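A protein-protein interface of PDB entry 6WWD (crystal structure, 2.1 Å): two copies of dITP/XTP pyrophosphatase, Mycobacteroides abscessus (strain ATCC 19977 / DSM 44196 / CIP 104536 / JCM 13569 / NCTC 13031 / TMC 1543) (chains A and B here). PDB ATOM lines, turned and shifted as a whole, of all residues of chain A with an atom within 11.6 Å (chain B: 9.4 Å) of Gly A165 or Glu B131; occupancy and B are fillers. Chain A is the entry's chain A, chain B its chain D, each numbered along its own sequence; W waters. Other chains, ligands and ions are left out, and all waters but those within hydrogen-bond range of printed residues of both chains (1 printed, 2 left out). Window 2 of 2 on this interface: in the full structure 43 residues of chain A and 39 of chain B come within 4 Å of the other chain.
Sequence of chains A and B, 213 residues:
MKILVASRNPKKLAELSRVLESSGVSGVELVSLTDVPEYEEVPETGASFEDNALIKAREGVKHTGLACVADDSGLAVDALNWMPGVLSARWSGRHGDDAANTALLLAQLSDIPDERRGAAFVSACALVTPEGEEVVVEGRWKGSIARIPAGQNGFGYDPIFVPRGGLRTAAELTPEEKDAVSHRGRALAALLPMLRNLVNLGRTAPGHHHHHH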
ATOM      1  N   ASP A 114      27.780   2.460   7.518  1.00  0.00           N
ATOM      2  CA  ASP A 114      27.416   2.611   8.928  1.00  0.00           C
ATOM      3  C   ASP A 114      27.459   4.060   9.381  1.00  0.00           C
ATOM      4  O   ASP A 114      26.612   4.498  10.162  1.00  0.00           O
ATOM      5  CB  ASP A 114      28.337   1.758   9.797  1.00  0.00           C
ATOM      6  CG  ASP A 114      28.063   0.266   9.654  1.00  0.00           C
ATOM      7  OD1 ASP A 114      29.025  -0.510   9.810  1.00  0.00           O
ATOM      8  OD2 ASP A 114      26.916  -0.135   9.336  1.00  0.00           O
ATOM      9  N   GLY A 118      22.701   6.934  10.774  1.00  0.00           N
ATOM     10  CA  GLY A 118      22.233   7.482  12.037  1.00  0.00           C
ATOM     11  C   GLY A 118      20.721   7.637  12.069  1.00  0.00           C
ATOM     12  O   GLY A 118      20.062   7.839  11.044  1.00  0.00           O
ATOM     13  N   ALA A 119      20.163   7.511  13.267  1.00  0.00           N
ATOM     14  CA  ALA A 119      18.721   7.596  13.429  1.00  0.00           C
ATOM     15  C   ALA A 119      18.421   7.884  14.887  1.00  0.00           C
ATOM     16  O   ALA A 119      19.311   7.848  15.743  1.00  0.00           O
ATOM     17  CB  ALA A 119      18.032   6.303  12.975  1.00  0.00           C
ATOM     18  N   TRP A 141      16.233   9.544  21.456  1.00  0.00           N
ATOM     19  CA  TRP A 141      17.174   8.487  21.841  1.00  0.00           C
ATOM     20  C   TRP A 141      18.022   8.163  20.619  1.00  0.00           C
ATOM     21  O   TRP A 141      17.523   7.584  19.655  1.00  0.00           O
ATOM     22  CB  TRP A 141      16.391   7.280  22.334  1.00  0.00           C
ATOM     23  CG  TRP A 141      17.139   6.138  22.888  1.00  0.00           C
ATOM     24  CD1 TRP A 141      18.395   6.134  23.401  1.00  0.00           C
ATOM     25  CD2 TRP A 141      16.656   4.788  22.972  1.00  0.00           C
ATOM     26  NE1 TRP A 141      18.729   4.856  23.815  1.00  0.00           N
ATOM     27  CE2 TRP A 141      17.673   4.014  23.564  1.00  0.00           C
ATOM     28  CE3 TRP A 141      15.453   4.161  22.605  1.00  0.00           C
ATOM     29  CZ2 TRP A 141      17.529   2.632  23.804  1.00  0.00           C
ATOM     30  CZ3 TRP A 141      15.310   2.785  22.839  1.00  0.00           C
ATOM     31  CH2 TRP A 141      16.349   2.040  23.431  1.00  0.00           C
ATOM     32  N   LYS A 142      19.297   8.540  20.652  1.00  0.00           N
ATOM     33  CA  LYS A 142      20.128   8.495  19.452  1.00  0.00           C
ATOM     34  C   LYS A 142      20.624   7.083  19.146  1.00  0.00           C
ATOM     35  O   LYS A 142      20.937   6.302  20.051  1.00  0.00           O
ATOM     36  CB  LYS A 142      21.326   9.448  19.587  1.00  0.00           C
ATOM     37  CG  LYS A 142      20.949  10.916  19.803  1.00  0.00           C
ATOM     38  CD  LYS A 142      20.098  11.397  18.621  1.00  0.00           C
ATOM     39  CE  LYS A 142      20.505  12.780  18.175  1.00  0.00           C
ATOM     40  NZ  LYS A 142      21.320  12.711  16.927  1.00  0.00           N
ATOM     41  N   GLY A 143      20.689   6.757  17.860  1.00  0.00           N
ATOM     42  CA  GLY A 143      21.203   5.466  17.441  1.00  0.00           C
ATOM     43  C   GLY A 143      21.445   5.367  15.950  1.00  0.00           C
ATOM     44  O   GLY A 143      21.830   6.341  15.291  1.00  0.00           O
ATOM     45  N   SER A 144      21.231   4.187  15.393  1.00  0.00           N
ATOM     46  CA  SER A 144      21.415   4.005  13.962  1.00  0.00           C
ATOM     47  C   SER A 144      20.567   2.816  13.542  1.00  0.00           C
ATOM     48  O   SER A 144      20.026   2.095  14.384  1.00  0.00           O
ATOM     49  CB  SER A 144      22.890   3.806  13.611  1.00  0.00           C
ATOM     50  OG  SER A 144      23.391   2.670  14.272  1.00  0.00           O
ATOM     51  N   ILE A 145      20.452   2.625  12.235  1.00  0.00           N
ATOM     52  CA  ILE A 145      19.631   1.549  11.690  1.00  0.00           C
ATOM     53  C   ILE A 145      20.517   0.340  11.425  1.00  0.00           C
ATOM     54  O   ILE A 145      21.533   0.443  10.727  1.00  0.00           O
ATOM     55  CB  ILE A 145      18.910   1.982  10.403  1.00  0.00           C
ATOM     56  CG1 ILE A 145      18.055   3.239  10.612  1.00  0.00           C
ATOM     57  CG2 ILE A 145      18.027   0.804   9.882  1.00  0.00           C
ATOM     58  CD1 ILE A 145      17.018   3.144  11.743  1.00  0.00           C
ATOM     59  N   PHE A 161      16.630  -0.900  15.288  1.00  0.00           N
ATOM     60  CA  PHE A 161      17.166   0.328  15.873  1.00  0.00           C
ATOM     61  C   PHE A 161      18.292  -0.034  16.827  1.00  0.00           C
ATOM     62  O   PHE A 161      18.058  -0.716  17.832  1.00  0.00           O
ATOM     63  CB  PHE A 161      16.091   1.124  16.614  1.00  0.00           C
ATOM     64  CG  PHE A 161      16.599   2.409  17.206  1.00  0.00           C
ATOM     65  CD1 PHE A 161      16.883   3.493  16.397  1.00  0.00           C
ATOM     66  CD2 PHE A 161      16.801   2.530  18.571  1.00  0.00           C
ATOM     67  CE1 PHE A 161      17.365   4.686  16.952  1.00  0.00           C
ATOM     68  CE2 PHE A 161      17.264   3.704  19.127  1.00  0.00           C
ATOM     69  CZ  PHE A 161      17.550   4.782  18.316  1.00  0.00           C
ATOM     70  N   VAL A 162      19.507   0.419  16.523  1.00  0.00           N
ATOM     71  CA  VAL A 162      20.668   0.156  17.364  1.00  0.00           C
ATOM     72  C   VAL A 162      20.949   1.417  18.181  1.00  0.00           C
ATOM     73  O   VAL A 162      21.484   2.396  17.622  1.00  0.00           O
ATOM     74  CB  VAL A 162      21.896  -0.247  16.542  1.00  0.00           C
ATOM     75  CG1 VAL A 162      23.084  -0.512  17.458  1.00  0.00           C
ATOM     76  CG2 VAL A 162      21.590  -1.473  15.645  1.00  0.00           C
ATOM     77  N   PRO A 163      20.623   1.447  19.468  1.00  0.00           N
ATOM     78  CA  PRO A 163      20.969   2.607  20.297  1.00  0.00           C
ATOM     79  C   PRO A 163      22.473   2.853  20.330  1.00  0.00           C
ATOM     80  O   PRO A 163      23.278   1.920  20.425  1.00  0.00           O
ATOM     81  CB  PRO A 163      20.444   2.220  21.685  1.00  0.00           C
ATOM     82  CG  PRO A 163      19.380   1.187  21.397  1.00  0.00           C
ATOM     83  CD  PRO A 163      19.915   0.412  20.239  1.00  0.00           C
ATOM     84  N   ARG A 164      22.830   4.130  20.207  1.00  0.00           N
ATOM     85  CA  ARG A 164      24.202   4.585  20.395  1.00  0.00           C
ATOM     86  C   ARG A 164      24.790   3.989  21.672  1.00  0.00           C
ATOM     87  O   ARG A 164      24.103   3.881  22.690  1.00  0.00           O
ATOM     88  CB  ARG A 164      24.214   6.119  20.477  1.00  0.00           C
ATOM     89  CG  ARG A 164      25.283   6.829  19.660  1.00  0.00           C
ATOM     90  CD  ARG A 164      24.802   7.158  18.239  1.00  0.00           C
ATOM     91  NE  ARG A 164      25.224   6.138  17.280  1.00  0.00           N
ATOM     92  CZ  ARG A 164      25.258   6.315  15.962  1.00  0.00           C
ATOM     93  NH1 ARG A 164      24.903   7.477  15.424  1.00  0.00           N
ATOM     94  NH2 ARG A 164      25.659   5.329  15.181  1.00  0.00           N
ATOM     95  N   GLY A 165      26.062   3.605  21.622  1.00  0.00           N
ATOM     96  CA  GLY A 165      26.691   3.039  22.793  1.00  0.00           C
ATOM     97  C   GLY A 165      26.679   1.521  22.891  1.00  0.00           C
ATOM     98  O   GLY A 165      27.168   0.977  23.889  1.00  0.00           O
ATOM     99  N   GLY A 166      26.128   0.820  21.906  1.00  0.00           N
ATOM    100  CA  GLY A 166      26.186  -0.628  21.927  1.00  0.00           C
ATOM    101  C   GLY A 166      25.940  -1.122  20.523  1.00  0.00           C
ATOM    102  O   GLY A 166      25.684  -0.343  19.598  1.00  0.00           O
ATOM    103  N   LEU A 167      26.008  -2.441  20.365  1.00  0.00           N
ATOM    104  CA  LEU A 167      25.766  -3.035  19.065  1.00  0.00           C
ATOM    105  C   LEU A 167      24.413  -3.716  18.971  1.00  0.00           C
ATOM    106  O   LEU A 167      23.952  -3.991  17.856  1.00  0.00           O
ATOM    107  CB  LEU A 167      26.866  -4.055  18.738  1.00  0.00           C
ATOM    108  CG  LEU A 167      28.298  -3.515  18.775  1.00  0.00           C
ATOM    109  CD1 LEU A 167      29.258  -4.646  18.425  1.00  0.00           C
ATOM    110  CD2 LEU A 167      28.473  -2.332  17.837  1.00  0.00           C
ATOM    111  N   ARG A 168      23.774  -3.982  20.109  1.00  0.00           N
ATOM    112  CA  ARG A 168      22.484  -4.651  20.138  1.00  0.00           C
ATOM    113  C   ARG A 168      21.365  -3.691  19.756  1.00  0.00           C
ATOM    114  O   ARG A 168      21.425  -2.486  20.033  1.00  0.00           O
ATOM    115  CB  ARG A 168      22.210  -5.222  21.530  1.00  0.00           C
ATOM    116  CG  ARG A 168      23.110  -6.367  21.962  1.00  0.00           C
ATOM    117  CD  ARG A 168      22.749  -6.782  23.393  1.00  0.00           C
ATOM    118  NE  ARG A 168      23.053  -5.711  24.325  1.00  0.00           N
ATOM    119  CZ  ARG A 168      22.564  -5.594  25.556  1.00  0.00           C
ATOM    120  NH1 ARG A 168      21.718  -6.490  26.040  1.00  0.00           N
ATOM    121  NH2 ARG A 168      22.935  -4.567  26.304  1.00  0.00           N
ATOM    122  N   THR A 169      20.320  -4.245  19.146  1.00  0.00           N
ATOM    123  CA  THR A 169      19.144  -3.464  18.811  1.00  0.00           C
ATOM    124  C   THR A 169      18.268  -3.286  20.051  1.00  0.00           C
ATOM    125  O   THR A 169      18.449  -3.972  21.062  1.00  0.00           O
ATOM    126  CB  THR A 169      18.348  -4.138  17.683  1.00  0.00           C
ATOM    127  OG1 THR A 169      17.724  -5.334  18.174  1.00  0.00           O
ATOM    128  CG2 THR A 169      19.277  -4.516  16.525  1.00  0.00           C
ATOM    129  N   ALA A 170      17.334  -2.323  19.974  1.00  0.00           N
ATOM    130  CA  ALA A 170      16.413  -2.089  21.088  1.00  0.00           C
ATOM    131  C   ALA A 170      15.646  -3.361  21.438  1.00  0.00           C
ATOM    132  O   ALA A 170      15.434  -3.661  22.617  1.00  0.00           O
ATOM    133  CB  ALA A 170      15.433  -0.963  20.745  1.00  0.00           C
ATOM    134  N   GLU A 172      16.749  -6.264  21.393  1.00  0.00           N
ATOM    135  CA  GLU A 172      17.633  -7.179  22.106  1.00  0.00           C
ATOM    136  C   GLU A 172      17.872  -6.760  23.553  1.00  0.00           C
ATOM    137  O   GLU A 172      18.507  -7.506  24.300  1.00  0.00           O
ATOM    138  CB  GLU A 172      18.968  -7.300  21.368  1.00  0.00           C
ATOM    139  CG  GLU A 172      18.886  -8.120  20.091  1.00  0.00           C
ATOM    140  CD  GLU A 172      20.220  -8.204  19.355  1.00  0.00           C
ATOM    141  OE1 GLU A 172      20.821  -7.154  19.054  1.00  0.00           O
ATOM    142  OE2 GLU A 172      20.672  -9.322  19.070  1.00  0.00           O
ATOM    143  N   LEU A 173      17.410  -5.576  23.950  1.00  0.00           N
ATOM    144  CA  LEU A 173      17.576  -5.074  25.305  1.00  0.00           C
ATOM    145  C   LEU A 173      16.614  -5.757  26.271  1.00  0.00           C
ATOM    146  O   LEU A 173      15.477  -6.088  25.921  1.00  0.00           O
ATOM    147  CB  LEU A 173      17.346  -3.562  25.353  1.00  0.00           C
ATOM    148  CG  LEU A 173      18.269  -2.736  24.464  1.00  0.00           C
ATOM    149  CD1 LEU A 173      17.966  -1.252  24.596  1.00  0.00           C
ATOM    150  CD2 LEU A 173      19.744  -3.048  24.766  1.00  0.00           C
ATOM    151  N   GLU A 177      16.889  -2.971  31.174  1.00  0.00           N
ATOM    152  CA  GLU A 177      17.611  -1.957  30.405  1.00  0.00           C
ATOM    153  C   GLU A 177      16.663  -0.954  29.760  1.00  0.00           C
ATOM    154  O   GLU A 177      16.939   0.250  29.750  1.00  0.00           O
ATOM    155  CB  GLU A 177      18.476  -2.619  29.339  1.00  0.00           C
ATOM    156  CG  GLU A 177      19.659  -3.369  29.891  1.00  0.00           C
ATOM    157  CD  GLU A 177      20.279  -4.282  28.863  1.00  0.00           C
ATOM    158  OE1 GLU A 177      19.530  -5.021  28.192  1.00  0.00           O
ATOM    159  OE2 GLU A 177      21.514  -4.254  28.718  1.00  0.00           O
ATOM    160  N   ALA A 180      15.564   1.853  32.112  1.00  0.00           N
ATOM    161  CA  ALA A 180      16.524   2.892  32.469  1.00  0.00           C
ATOM    162  C   ALA A 180      16.620   4.002  31.428  1.00  0.00           C
ATOM    163  O   ALA A 180      17.095   5.094  31.756  1.00  0.00           O
ATOM    164  CB  ALA A 180      17.905   2.273  32.688  1.00  0.00           C
ATOM    165  N   VAL A 181      16.187   3.752  30.190  1.00  0.00           N
ATOM    166  CA  VAL A 181      16.268   4.767  29.140  1.00  0.00           C
ATOM    167  C   VAL A 181      15.096   5.749  29.230  1.00  0.00           C
ATOM    168  O   VAL A 181      15.254   6.950  28.976  1.00  0.00           O
ATOM    169  CB  VAL A 181      16.352   4.077  27.764  1.00  0.00           C
ATOM    170  CG1 VAL A 181      16.183   5.076  26.634  1.00  0.00           C
ATOM    171  CG2 VAL A 181      17.682   3.343  27.632  1.00  0.00           C
ATOM    172  N   ARG A 184      15.927   8.064  32.384  1.00  0.00           N
ATOM    173  CA  ARG A 184      16.845   9.152  32.065  1.00  0.00           C
ATOM    174  C   ARG A 184      16.215  10.180  31.131  1.00  0.00           C
ATOM    175  O   ARG A 184      16.508  11.378  31.248  1.00  0.00           O
ATOM    176  CB  ARG A 184      18.124   8.583  31.452  1.00  0.00           C
ATOM    177  N   MET B   1      27.611   7.605  43.014  1.00  0.00           N
ATOM    178  CA  MET B   1      27.991   7.788  41.618  1.00  0.00           C
ATOM    179  C   MET B   1      28.165   9.271  41.290  1.00  0.00           C
ATOM    180  O   MET B   1      27.333  10.095  41.676  1.00  0.00           O
ATOM    181  CB  MET B   1      26.932   7.160  40.705  1.00  0.00           C
ATOM    182  CG  MET B   1      26.771   7.837  39.355  1.00  0.00           C
ATOM    183  SD  MET B   1      25.557   7.017  38.299  1.00  0.00           S
ATOM    184  CE  MET B   1      26.401   5.471  37.942  1.00  0.00           C
ATOM    185  N   VAL B  61      31.978  13.637  28.807  1.00  0.00           N
ATOM    186  CA  VAL B  61      32.320  12.225  28.996  1.00  0.00           C
ATOM    187  C   VAL B  61      33.742  11.962  28.522  1.00  0.00           C
ATOM    188  O   VAL B  61      34.512  11.232  29.166  1.00  0.00           O
ATOM    189  CB  VAL B  61      31.305  11.322  28.273  1.00  0.00           C
ATOM    190  CG1 VAL B  61      31.661   9.839  28.468  1.00  0.00           C
ATOM    191  CG2 VAL B  61      29.882  11.609  28.770  1.00  0.00           C
ATOM    192  N   GLY B  65      35.228  10.440  31.745  1.00  0.00           N
ATOM    193  CA  GLY B  65      34.655   9.123  31.899  1.00  0.00           C
ATOM    194  C   GLY B  65      33.377   9.072  32.702  1.00  0.00           C
ATOM    195  O   GLY B  65      32.811   7.981  32.857  1.00  0.00           O
ATOM    196  N   LEU B  66      32.887  10.219  33.178  1.00  0.00           N
ATOM    197  CA  LEU B  66      31.632  10.313  33.898  1.00  0.00           C
ATOM    198  C   LEU B  66      30.482  10.551  32.933  1.00  0.00           C
ATOM    199  O   LEU B  66      30.648  11.158  31.873  1.00  0.00           O
ATOM    200  CB  LEU B  66      31.682  11.458  34.913  1.00  0.00           C
ATOM    201  CG  LEU B  66      32.849  11.396  35.916  1.00  0.00           C
ATOM    202  CD1 LEU B  66      32.917  12.663  36.767  1.00  0.00           C
ATOM    203  CD2 LEU B  66      32.709  10.157  36.774  1.00  0.00           C
ATOM    204  N   ALA B  67      29.307  10.061  33.307  1.00  0.00           N
ATOM    205  CA  ALA B  67      28.092  10.508  32.660  1.00  0.00           C
ATOM    206  C   ALA B  67      28.027  12.029  32.734  1.00  0.00           C
ATOM    207  O   ALA B  67      28.433  12.641  33.730  1.00  0.00           O
ATOM    208  CB  ALA B  67      26.879   9.863  33.333  1.00  0.00           C
ATOM    209  N   CYS B  68      27.567  12.654  31.660  1.00  0.00           N
ATOM    210  CA  CYS B  68      27.625  14.101  31.577  1.00  0.00           C
ATOM    211  C   CYS B  68      26.284  14.628  31.111  1.00  0.00           C
ATOM    212  O   CYS B  68      25.745  14.158  30.113  1.00  0.00           O
ATOM    213  CB  CYS B  68      28.737  14.588  30.634  1.00  0.00           C
ATOM    214  SG  CYS B  68      28.676  16.390  30.483  1.00  0.00           S
ATOM    215  N   LEU B 127      22.097  14.045  27.839  1.00  0.00           N
ATOM    216  CA  LEU B 127      22.829  13.118  28.686  1.00  0.00           C
ATOM    217  C   LEU B 127      23.593  12.162  27.791  1.00  0.00           C
ATOM    218  O   LEU B 127      23.015  11.577  26.870  1.00  0.00           O
ATOM    219  CB  LEU B 127      21.903  12.329  29.612  1.00  0.00           C
ATOM    220  CG  LEU B 127      22.560  11.106  30.296  1.00  0.00           C
ATOM    221  CD1 LEU B 127      23.546  11.512  31.374  1.00  0.00           C
ATOM    222  CD2 LEU B 127      21.512  10.136  30.850  1.00  0.00           C
ATOM    223  N   VAL B 128      24.880  12.000  28.067  1.00  0.00           N
ATOM    224  CA  VAL B 128      25.707  10.977  27.433  1.00  0.00           C
ATOM    225  C   VAL B 128      26.337  10.172  28.556  1.00  0.00           C
ATOM    226  O   VAL B 128      26.884  10.741  29.510  1.00  0.00           O
ATOM    227  CB  VAL B 128      26.784  11.578  26.510  1.00  0.00           C
ATOM    228  CG1 VAL B 128      27.644  10.483  25.907  1.00  0.00           C
ATOM    229  CG2 VAL B 128      26.138  12.417  25.412  1.00  0.00           C
ATOM    230  N   THR B 129      26.203   8.882  28.479  1.00  0.00           N
ATOM    231  CA  THR B 129      26.690   7.994  29.520  1.00  0.00           C
ATOM    232  C   THR B 129      28.108   7.551  29.206  1.00  0.00           C
ATOM    233  O   THR B 129      28.572   7.668  28.065  1.00  0.00           O
ATOM    234  CB  THR B 129      25.772   6.775  29.640  1.00  0.00           C
ATOM    235  OG1 THR B 129      25.890   5.968  28.460  1.00  0.00           O
ATOM    236  CG2 THR B 129      24.316   7.214  29.850  1.00  0.00           C
ATOM    237  N   PRO B 130      28.831   7.029  30.201  1.00  0.00           N
ATOM    238  CA  PRO B 130      30.178   6.516  29.919  1.00  0.00           C
ATOM    239  C   PRO B 130      30.201   5.437  28.842  1.00  0.00           C
ATOM    240  O   PRO B 130      31.199   5.302  28.121  1.00  0.00           O
ATOM    241  CB  PRO B 130      30.633   5.963  31.282  1.00  0.00           C
ATOM    242  CG  PRO B 130      29.819   6.694  32.288  1.00  0.00           C
ATOM    243  CD  PRO B 130      28.484   6.913  31.629  1.00  0.00           C
ATOM    244  N   GLU B 131      29.140   4.642  28.730  1.00  0.00           N
ATOM    245  CA  GLU B 131      29.077   3.587  27.726  1.00  0.00           C
ATOM    246  C   GLU B 131      28.726   4.105  26.334  1.00  0.00           C
ATOM    247  O   GLU B 131      28.712   3.314  25.382  1.00  0.00           O
ATOM    248  CB  GLU B 131      28.061   2.525  28.156  1.00  0.00           C
ATOM    249  CG  GLU B 131      28.372   1.853  29.510  1.00  0.00           C
ATOM    250  CD  GLU B 131      27.980   2.708  30.714  1.00  0.00           C
ATOM    251  OE1 GLU B 131      27.318   3.747  30.524  1.00  0.00           O
ATOM    252  OE2 GLU B 131      28.332   2.333  31.857  1.00  0.00           O
ATOM    253  N   GLY B 132      28.437   5.397  26.195  1.00  0.00           N
ATOM    254  CA  GLY B 132      28.137   6.001  24.912  1.00  0.00           C
ATOM    255  C   GLY B 132      26.670   6.142  24.557  1.00  0.00           C
ATOM    256  O   GLY B 132      26.363   6.519  23.419  1.00  0.00           O
ATOM    257  N   GLU B 133      25.758   5.885  25.490  1.00  0.00           N
ATOM    258  CA  GLU B 133      24.349   6.177  25.250  1.00  0.00           C
ATOM    259  C   GLU B 133      24.117   7.686  25.163  1.00  0.00           C
ATOM    260  O   GLU B 133      24.718   8.465  25.910  1.00  0.00           O
ATOM    261  CB  GLU B 133      23.508   5.592  26.378  1.00  0.00           C
ATOM    262  CG  GLU B 133      22.034   5.955  26.304  1.00  0.00           C
ATOM    263  CD  GLU B 133      21.212   5.261  27.388  1.00  0.00           C
ATOM    264  OE1 GLU B 133      21.102   4.021  27.359  1.00  0.00           O
ATOM    265  OE2 GLU B 133      20.692   5.971  28.276  1.00  0.00           O
ATOM    266  N   GLU B 134      23.243   8.108  24.246  1.00  0.00           N
ATOM    267  CA  GLU B 134      22.960   9.536  24.056  1.00  0.00           C
ATOM    268  C   GLU B 134      21.460   9.761  24.073  1.00  0.00           C
ATOM    269  O   GLU B 134      20.733   9.151  23.287  1.00  0.00           O
ATOM    270  CB  GLU B 134      23.509  10.064  22.730  1.00  0.00           C
ATOM    271  CG  GLU B 134      24.976   9.819  22.520  1.00  0.00           C
ATOM    272  CD  GLU B 134      25.474  10.452  21.241  1.00  0.00           C
ATOM    273  OE1 GLU B 134      24.627  10.933  20.455  1.00  0.00           O
ATOM    274  OE2 GLU B 134      26.705  10.475  21.029  1.00  0.00           O
ATOM    275  N   VAL B 135      21.002  10.656  24.944  1.00  0.00           N
ATOM    276  CA  VAL B 135      19.612  11.081  24.980  1.00  0.00           C
ATOM    277  C   VAL B 135      19.584  12.602  25.044  1.00  0.00           C
ATOM    278  O   VAL B 135      20.315  13.215  25.828  1.00  0.00           O
ATOM    279  CB  VAL B 135      18.856  10.493  26.191  1.00  0.00           C
ATOM    280  CG1 VAL B 135      17.411  10.995  26.189  1.00  0.00           C
ATOM    281  CG2 VAL B 135      18.920   8.959  26.206  1.00  0.00           C
HETATM  282  O   HOH W   1      21.671   5.918  22.766  1.00  0.00           O
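Of chain B, only Glu B131 (3.2 Å) and Gly B132 (3.4 Å) come within 4 Å of Gly A165. Of chain A, only Gly A165 comes within 4 Å of Glu B131. No residue of chain A comes within 4 Å of Thr B129. No residue of chain A comes within 4 Å of Pro B130. Printed residues of chain B within 4 Å of Lys A142: Glu B134. Of the printed residues of chain B, Val A181 touches Glu B133. Of the printed residues of chain B, Arg A184 touches Leu B127 (3.8 Å). Of the printed residues of chain A, Leu B127 touches Arg A184 (3.8 Å). Gly A143 touches none of the printed residues of chain B.
Water W1 lies within hydrogen-bond range of the backbone carbonyl oxygen (O) of Lys A142 (2.8 Å), the backbone NH (N) of Glu B134 (3.1 Å), the backbone carbonyl oxygen (O) of Arg A164 (3.2 Å) and the indole nitrogen (NE1) of Trp A141 (3.3 Å).
No position is printed for both chains. Of the 9 pairs that touch across the chains among the printed residues, none has its exchanged pair printed and touching as well.
The backbone NH (N) of Lys A142 is in hydrogen-bond range of the backbone carbonyl oxygen (O) of Glu B134, at 3.1 Å. N of Gly A165 lies within hydrogen-bond range of O of Gly B132 (3.4 Å). O of Gly A165 sits close to O of Glu B131 (3.2 Å).
Among the printed residues, pairs that only touch across the chains: Trp A141 with Glu B134 (3.8 Å), Arg A164 with Gly B132 (3.5 Å), Arg A164 with Glu B133 (3.4 Å), Arg A164 with Glu B134 (3.96 Å), Val A181 with Glu B133 (3.5 Å) and Arg A184 with Leu B127 (3.8 Å).
Along chain A the printed residues that touch a printed residue of chain B span positions 141 to 184. Of the 15 printed residues of chain B, 5 touch a printed residue of chain A. Hydrophobic or aromatic side chains of chain B within 4 Å of the printed part of chain A: Leu B127. Among the printed residues, 9 pairs touch across the chains.
The backbone NH (N) of Arg A164 is in hydrogen-bond range of the backbone carbonyl oxygen (O) of Lys A142 (2.9 Å). NH1 of Arg A164 sits at hydrogen-bond distance from O of Gly A143 (3.3 Å). N of Leu B127 sits at hydrogen-bond distance from O of Val B135, at 2.8 Å. The side-chain hydroxyl (OG1) of Thr B129 is in hydrogen-bond range of the side-chain carboxylate (OE1) of Glu B131, at 3.4 Å. The backbone NH (N) of Gly B132 is in hydrogen-bond range of the side-chain hydroxyl (OG1) of Thr B129 (3.5 Å). OG1 of Thr B129 lies within hydrogen-bond range of N of Glu B133, at 3.0 Å.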
